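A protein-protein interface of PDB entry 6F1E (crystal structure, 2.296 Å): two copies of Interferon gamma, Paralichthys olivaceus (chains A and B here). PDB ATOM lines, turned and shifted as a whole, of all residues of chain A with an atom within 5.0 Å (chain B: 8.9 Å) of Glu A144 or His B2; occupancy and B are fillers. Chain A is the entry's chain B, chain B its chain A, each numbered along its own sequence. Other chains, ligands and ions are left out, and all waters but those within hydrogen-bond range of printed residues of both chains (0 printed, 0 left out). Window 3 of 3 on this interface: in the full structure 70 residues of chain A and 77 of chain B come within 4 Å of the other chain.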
ATOM      1  N   LEU A 139      -4.804   6.370   7.354  1.00  0.00           N
ATOM      2  CA  LEU A 139      -4.018   5.417   8.143  1.00  0.00           C
ATOM      3  C   LEU A 139      -3.352   6.014   9.372  1.00  0.00           C
ATOM      4  O   LEU A 139      -3.276   5.374  10.394  1.00  0.00           O
ATOM      5  CB  LEU A 139      -2.999   4.658   7.277  1.00  0.00           C
ATOM      6  CG  LEU A 139      -2.143   3.567   7.967  1.00  0.00           C
ATOM      7  CD1 LEU A 139      -2.906   2.570   8.874  1.00  0.00           C
ATOM      8  CD2 LEU A 139      -1.378   2.792   6.901  1.00  0.00           C
ATOM      9  N   GLN A 140      -2.874   7.235   9.301  1.00  0.00           N
ATOM     10  CA  GLN A 140      -2.049   7.774  10.409  1.00  0.00           C
ATOM     11  C   GLN A 140      -2.893   7.939  11.658  1.00  0.00           C
ATOM     12  O   GLN A 140      -2.536   7.448  12.736  1.00  0.00           O
ATOM     13  CB  GLN A 140      -1.419   9.108  10.018  1.00  0.00           C
ATOM     14  CG  GLN A 140      -0.080   9.368  10.683  1.00  0.00           C
ATOM     15  CD  GLN A 140       0.605  10.607  10.126  1.00  0.00           C
ATOM     16  OE1 GLN A 140       0.880  10.694   8.912  1.00  0.00           O
ATOM     17  NE2 GLN A 140       0.870  11.579  11.002  1.00  0.00           N
ATOM     18  N   TRP A 141      -4.042   8.591  11.486  1.00  0.00           N
ATOM     19  CA  TRP A 141      -4.959   8.758  12.578  1.00  0.00           C
ATOM     20  C   TRP A 141      -5.440   7.384  13.077  1.00  0.00           C
ATOM     21  O   TRP A 141      -5.479   7.126  14.292  1.00  0.00           O
ATOM     22  CB  TRP A 141      -6.150   9.625  12.172  1.00  0.00           C
ATOM     23  CG  TRP A 141      -6.936   9.986  13.339  1.00  0.00           C
ATOM     24  CD1 TRP A 141      -6.775  11.093  14.128  1.00  0.00           C
ATOM     25  CD2 TRP A 141      -7.982   9.205  13.935  1.00  0.00           C
ATOM     26  NE1 TRP A 141      -7.685  11.063  15.162  1.00  0.00           N
ATOM     27  CE2 TRP A 141      -8.432   9.916  15.075  1.00  0.00           C
ATOM     28  CE3 TRP A 141      -8.592   7.980  13.606  1.00  0.00           C
ATOM     29  CZ2 TRP A 141      -9.466   9.453  15.885  1.00  0.00           C
ATOM     30  CZ3 TRP A 141      -9.622   7.507  14.420  1.00  0.00           C
ATOM     31  CH2 TRP A 141     -10.041   8.241  15.553  1.00  0.00           C
ATOM     32  N   MET A 142      -5.808   6.508  12.141  1.00  0.00           N
ATOM     33  CA  MET A 142      -6.361   5.216  12.509  1.00  0.00           C
ATOM     34  C   MET A 142      -5.353   4.394  13.317  1.00  0.00           C
ATOM     35  O   MET A 142      -5.723   3.785  14.340  1.00  0.00           O
ATOM     36  CB  MET A 142      -6.898   4.488  11.284  1.00  0.00           C
ATOM     37  CG  MET A 142      -8.213   5.097  10.752  1.00  0.00           C
ATOM     38  SD  MET A 142      -9.579   4.710  11.863  1.00  0.00           S
ATOM     39  CE  MET A 142     -10.921   5.745  11.301  1.00  0.00           C
ATOM     40  N   TYR A 143      -4.079   4.443  12.940  1.00  0.00           N
ATOM     41  CA  TYR A 143      -3.040   3.694  13.682  1.00  0.00           C
ATOM     42  C   TYR A 143      -2.694   4.337  15.022  1.00  0.00           C
ATOM     43  O   TYR A 143      -2.391   3.614  15.972  1.00  0.00           O
ATOM     44  CB  TYR A 143      -1.793   3.549  12.845  1.00  0.00           C
ATOM     45  CG  TYR A 143      -0.771   2.539  13.329  1.00  0.00           C
ATOM     46  CD1 TYR A 143       0.279   2.915  14.134  1.00  0.00           C
ATOM     47  CD2 TYR A 143      -0.789   1.222  12.874  1.00  0.00           C
ATOM     48  CE1 TYR A 143       1.255   1.998  14.545  1.00  0.00           C
ATOM     49  CE2 TYR A 143       0.192   0.308  13.244  1.00  0.00           C
ATOM     50  CZ  TYR A 143       1.219   0.702  14.085  1.00  0.00           C
ATOM     51  OH  TYR A 143       2.196  -0.212  14.482  1.00  0.00           O
ATOM     52  N   GLU A 144      -2.739   5.673  15.108  1.00  0.00           N
ATOM     53  CA  GLU A 144      -2.640   6.366  16.418  1.00  0.00           C
ATOM     54  C   GLU A 144      -3.726   5.812  17.342  1.00  0.00           C
ATOM     55  O   GLU A 144      -3.420   5.275  18.396  1.00  0.00           O
ATOM     56  CB  GLU A 144      -2.805   7.897  16.280  1.00  0.00           C
ATOM     57  CG  GLU A 144      -1.751   8.757  16.995  1.00  0.00           C
ATOM     58  CD  GLU A 144      -2.309   9.579  18.165  1.00  0.00           C
ATOM     59  OE1 GLU A 144      -2.456   9.021  19.285  1.00  0.00           O
ATOM     60  OE2 GLU A 144      -2.583  10.794  17.961  1.00  0.00           O
ATOM     61  N   GLU A 145      -4.983   5.879  16.895  1.00  0.00           N
ATOM     62  CA  GLU A 145      -6.147   5.497  17.690  1.00  0.00           C
ATOM     63  C   GLU A 145      -6.082   4.043  18.126  1.00  0.00           C
ATOM     64  O   GLU A 145      -6.213   3.759  19.310  1.00  0.00           O
ATOM     65  CB  GLU A 145      -7.431   5.767  16.897  1.00  0.00           C
ATOM     66  CG  GLU A 145      -8.752   5.451  17.593  1.00  0.00           C
ATOM     67  CD  GLU A 145      -9.032   6.286  18.843  1.00  0.00           C
ATOM     68  OE1 GLU A 145      -8.133   7.012  19.304  1.00  0.00           O
ATOM     69  OE2 GLU A 145     -10.171   6.203  19.374  1.00  0.00           O
ATOM     70  N   ALA A 146      -5.836   3.134  17.180  1.00  0.00           N
ATOM     71  CA  ALA A 146      -5.689   1.723  17.496  1.00  0.00           C
ATOM     72  C   ALA A 146      -4.628   1.473  18.550  1.00  0.00           C
ATOM     73  O   ALA A 146      -4.898   0.793  19.551  1.00  0.00           O
ATOM     74  CB  ALA A 146      -5.379   0.919  16.248  1.00  0.00           C
ATOM     75  N   SER A 147      -3.428   1.999  18.315  1.00  0.00           N
ATOM     76  CA  SER A 147      -2.329   1.934  19.299  1.00  0.00           C
ATOM     77  C   SER A 147      -2.708   2.410  20.683  1.00  0.00           C
ATOM     78  O   SER A 147      -2.414   1.734  21.632  1.00  0.00           O
ATOM     79  CB  SER A 147      -1.125   2.739  18.844  1.00  0.00           C
ATOM     80  OG  SER A 147      -0.612   2.159  17.660  1.00  0.00           O
ATOM     81  N   SER A 148      -3.370   3.553  20.804  1.00  0.00           N
ATOM     82  CA  SER A 148      -3.661   4.107  22.143  1.00  0.00           C
ATOM     83  C   SER A 148      -4.747   3.290  22.893  1.00  0.00           C
ATOM     84  O   SER A 148      -4.731   3.173  24.113  1.00  0.00           O
ATOM     85  CB  SER A 148      -4.021   5.614  22.051  1.00  0.00           C
ATOM     86  OG  SER A 148      -5.257   5.838  21.395  1.00  0.00           O
ATOM     87  N   HIS B   2       3.961   9.691  18.919  1.00  0.00           N
ATOM     88  CA  HIS B   2       2.698   8.923  19.187  1.00  0.00           C
ATOM     89  C   HIS B   2       2.461   7.776  18.194  1.00  0.00           C
ATOM     90  O   HIS B   2       1.873   6.743  18.552  1.00  0.00           O
ATOM     91  CB  HIS B   2       1.493   9.863  19.234  1.00  0.00           C
ATOM     92  CG  HIS B   2       1.448  10.711  20.468  1.00  0.00           C
ATOM     93  ND1 HIS B   2       1.759  12.054  20.460  1.00  0.00           N
ATOM     94  CD2 HIS B   2       1.144  10.402  21.751  1.00  0.00           C
ATOM     95  CE1 HIS B   2       1.636  12.541  21.682  1.00  0.00           C
ATOM     96  NE2 HIS B   2       1.264  11.559  22.484  1.00  0.00           N
ATOM     97  N   ILE B   3       2.883   7.978  16.945  1.00  0.00           N
ATOM     98  CA  ILE B   3       3.195   6.865  16.028  1.00  0.00           C
ATOM     99  C   ILE B   3       4.683   6.972  15.757  1.00  0.00           C
ATOM    100  O   ILE B   3       5.272   8.026  16.028  1.00  0.00           O
ATOM    101  CB  ILE B   3       2.409   6.908  14.696  1.00  0.00           C
ATOM    102  CG1 ILE B   3       2.627   8.230  13.945  1.00  0.00           C
ATOM    103  CG2 ILE B   3       0.925   6.694  14.956  1.00  0.00           C
ATOM    104  CD1 ILE B   3       2.416   8.118  12.456  1.00  0.00           C
ATOM    105  N   PRO B   4       5.305   5.899  15.233  1.00  0.00           N
ATOM    106  CA  PRO B   4       6.733   6.042  14.873  1.00  0.00           C
ATOM    107  C   PRO B   4       6.958   7.094  13.782  1.00  0.00           C
ATOM    108  O   PRO B   4       6.108   7.275  12.892  1.00  0.00           O
ATOM    109  CB  PRO B   4       7.142   4.641  14.387  1.00  0.00           C
ATOM    110  CG  PRO B   4       6.053   3.711  14.837  1.00  0.00           C
ATOM    111  CD  PRO B   4       4.803   4.524  15.038  1.00  0.00           C
ATOM    112  N   ALA B   5       8.085   7.799  13.877  1.00  0.00           N
ATOM    113  CA  ALA B   5       8.479   8.783  12.863  1.00  0.00           C
ATOM    114  C   ALA B   5       8.447   8.119  11.493  1.00  0.00           C
ATOM    115  O   ALA B   5       7.966   8.715  10.519  1.00  0.00           O
ATOM    116  CB  ALA B   5       9.876   9.345  13.159  1.00  0.00           C
ATOM    117  N   MET B   7       6.776   5.556  10.343  1.00  0.00           N
ATOM    118  CA  MET B   7       5.414   5.366   9.843  1.00  0.00           C
ATOM    119  C   MET B   7       4.937   6.623   9.142  1.00  0.00           C
ATOM    120  O   MET B   7       4.470   6.546   7.994  1.00  0.00           O
ATOM    121  CB  MET B   7       4.462   5.036  10.994  1.00  0.00           C
ATOM    122  CG  MET B   7       3.088   4.555  10.570  1.00  0.00           C
ATOM    123  SD  MET B   7       3.152   2.806  10.188  1.00  0.00           S
ATOM    124  CE  MET B   7       1.404   2.443  10.155  1.00  0.00           C
ATOM    125  N   ASN B   8       5.058   7.770   9.837  1.00  0.00           N
ATOM    126  CA  ASN B   8       4.602   9.070   9.300  1.00  0.00           C
ATOM    127  C   ASN B   8       5.344   9.358   8.014  1.00  0.00           C
ATOM    128  O   ASN B   8       4.750   9.625   6.989  1.00  0.00           O
ATOM    129  CB  ASN B   8       4.822  10.231  10.297  1.00  0.00           C
ATOM    130  CG  ASN B   8       4.580  11.620   9.663  1.00  0.00           C
ATOM    131  OD1 ASN B   8       3.448  12.117   9.636  1.00  0.00           O
ATOM    132  ND2 ASN B   8       5.654  12.251   9.147  1.00  0.00           N
ATOM    133  N   ILE B  11       4.419   7.040   5.190  1.00  0.00           N
ATOM    134  CA  ILE B  11       3.080   7.321   4.630  1.00  0.00           C
ATOM    135  C   ILE B  11       3.123   8.496   3.661  1.00  0.00           C
ATOM    136  O   ILE B  11       2.573   8.414   2.546  1.00  0.00           O
ATOM    137  CB  ILE B  11       2.010   7.583   5.724  1.00  0.00           C
ATOM    138  CG1 ILE B  11       1.558   6.257   6.355  1.00  0.00           C
ATOM    139  CG2 ILE B  11       0.790   8.343   5.158  1.00  0.00           C
ATOM    140  CD1 ILE B  11       0.778   6.429   7.656  1.00  0.00           C
ATOM    141  N   MET B  48     -12.107  -1.078  15.672  1.00  0.00           N
ATOM    142  CA  MET B  48     -10.689  -0.834  15.324  1.00  0.00           C
ATOM    143  C   MET B  48      -9.973  -2.052  14.787  1.00  0.00           C
ATOM    144  O   MET B  48      -9.169  -1.931  13.849  1.00  0.00           O
ATOM    145  CB  MET B  48      -9.867  -0.319  16.503  1.00  0.00           C
ATOM    146  CG  MET B  48      -9.402   1.124  16.435  1.00  0.00           C
ATOM    147  SD  MET B  48      -8.914   1.771  14.809  1.00  0.00           S
ATOM    148  CE  MET B  48     -10.442   2.699  14.624  1.00  0.00           C
ATOM    149  N   LEU B  52      -8.231  -2.392  11.075  1.00  0.00           N
ATOM    150  CA  LEU B  52      -6.882  -2.910  10.846  1.00  0.00           C
ATOM    151  C   LEU B  52      -6.914  -4.104   9.872  1.00  0.00           C
ATOM    152  O   LEU B  52      -6.060  -4.175   8.972  1.00  0.00           O
ATOM    153  CB  LEU B  52      -6.185  -3.270  12.172  1.00  0.00           C
ATOM    154  CG  LEU B  52      -5.854  -2.103  13.127  1.00  0.00           C
ATOM    155  CD1 LEU B  52      -5.397  -2.612  14.501  1.00  0.00           C
ATOM    156  CD2 LEU B  52      -4.768  -1.222  12.541  1.00  0.00           C
ATOM    157  N   LEU B 103       0.497  -5.156  14.783  1.00  0.00           N
ATOM    158  CA  LEU B 103      -0.373  -4.543  15.791  1.00  0.00           C
ATOM    159  C   LEU B 103      -1.623  -5.427  16.011  1.00  0.00           C
ATOM    160  O   LEU B 103      -2.089  -5.645  17.148  1.00  0.00           O
ATOM    161  CB  LEU B 103      -0.759  -3.128  15.367  1.00  0.00           C
ATOM    162  CG  LEU B 103      -1.637  -2.327  16.332  1.00  0.00           C
ATOM    163  CD1 LEU B 103      -1.067  -2.221  17.730  1.00  0.00           C
ATOM    164  CD2 LEU B 103      -1.769  -0.931  15.805  1.00  0.00           C
ATOM    165  N   PHE B 108      -4.913  -7.409  19.033  1.00  0.00           N
ATOM    166  CA  PHE B 108      -6.262  -7.599  18.530  1.00  0.00           C
ATOM    167  C   PHE B 108      -6.561  -9.076  18.209  1.00  0.00           C
ATOM    168  O   PHE B 108      -7.088  -9.396  17.141  1.00  0.00           O
ATOM    169  CB  PHE B 108      -6.462  -6.649  17.310  1.00  0.00           C
ATOM    170  CG  PHE B 108      -6.533  -5.174  17.703  1.00  0.00           C
ATOM    171  CD1 PHE B 108      -7.747  -4.590  18.076  1.00  0.00           C
ATOM    172  CD2 PHE B 108      -5.371  -4.378  17.747  1.00  0.00           C
ATOM    173  CE1 PHE B 108      -7.816  -3.253  18.477  1.00  0.00           C
ATOM    174  CE2 PHE B 108      -5.438  -3.038  18.134  1.00  0.00           C
ATOM    175  CZ  PHE B 108      -6.665  -2.476  18.511  1.00  0.00           C
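OD1 of Asn B8 lies within hydrogen-bond range of NE2 of Gln A140, 3.0 Å away.
Of chain B, only His B2 (3.96 Å) and Ile B3 (3.8 Å) come within 4 Å of Glu A144. His B2 touches just one residue of chain A: Glu A144 (3.96 Å). Printed residues of chain B within 4 Å of Ser A147: Leu B103 (3.8 Å). Printed residues of chain A within 4 Å of Leu B52: Ala A146. Of the printed residues of chain A, Leu B103 touches Tyr A143 and Ser A147. Of the printed residues of chain B, Gln A140 touches Ile B3 (3.3 Å) and Asn B8 (3.0 Å). The nearest residue of chain B that does not touch Glu A144 is Leu B103 (6.7 Å).
Ile B3 touches Gln A140. SD of Met A142 touches CE of Met B48, 3.5 Å away. Ile B3 touches Tyr A143. Tyr A143 touches Met B7 (CD2 to CE, 3.7 Å). CE2 of Tyr A143 touches CD2 of Leu B103, at 3.5 Å. His B2 touches Glu A144 (CB to CD, 3.96 Å). Met B48 touches Ala A146 (CG to CA, 3.9 Å). Leu B52 touches Ala A146 (CD1 to CB, 3.9 Å). Phe B108 touches Ala A146 (CZ to O, 3.9 Å). Leu B103 touches Ser A147.
The side-chain hydroxyl (OG) of Ser A147 is in hydrogen-bond range of the backbone carbonyl oxygen (O) of Tyr A143 (2.9 Å).
No position is printed for both chains.
Of the 10 printed residues of chain A, 6 touch a printed residue of chain B. Hydrophobic or aromatic side chains of chain A within 4 Å of the printed part of chain B: Met A142, Tyr A143 and Ala A146. Printed residues of chain B that touch a printed residue of chain A: His B2, Ile B3, Met B7, Asn B8, Met B48, Leu B52, Leu B103 and Phe B108. Among the printed residues, 12 pairs touch across the chains. Among the printed residues, no Asp or Glu carboxylate lies within 4 Å of a Lys or Arg side-chain nitrogen of the other chain.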
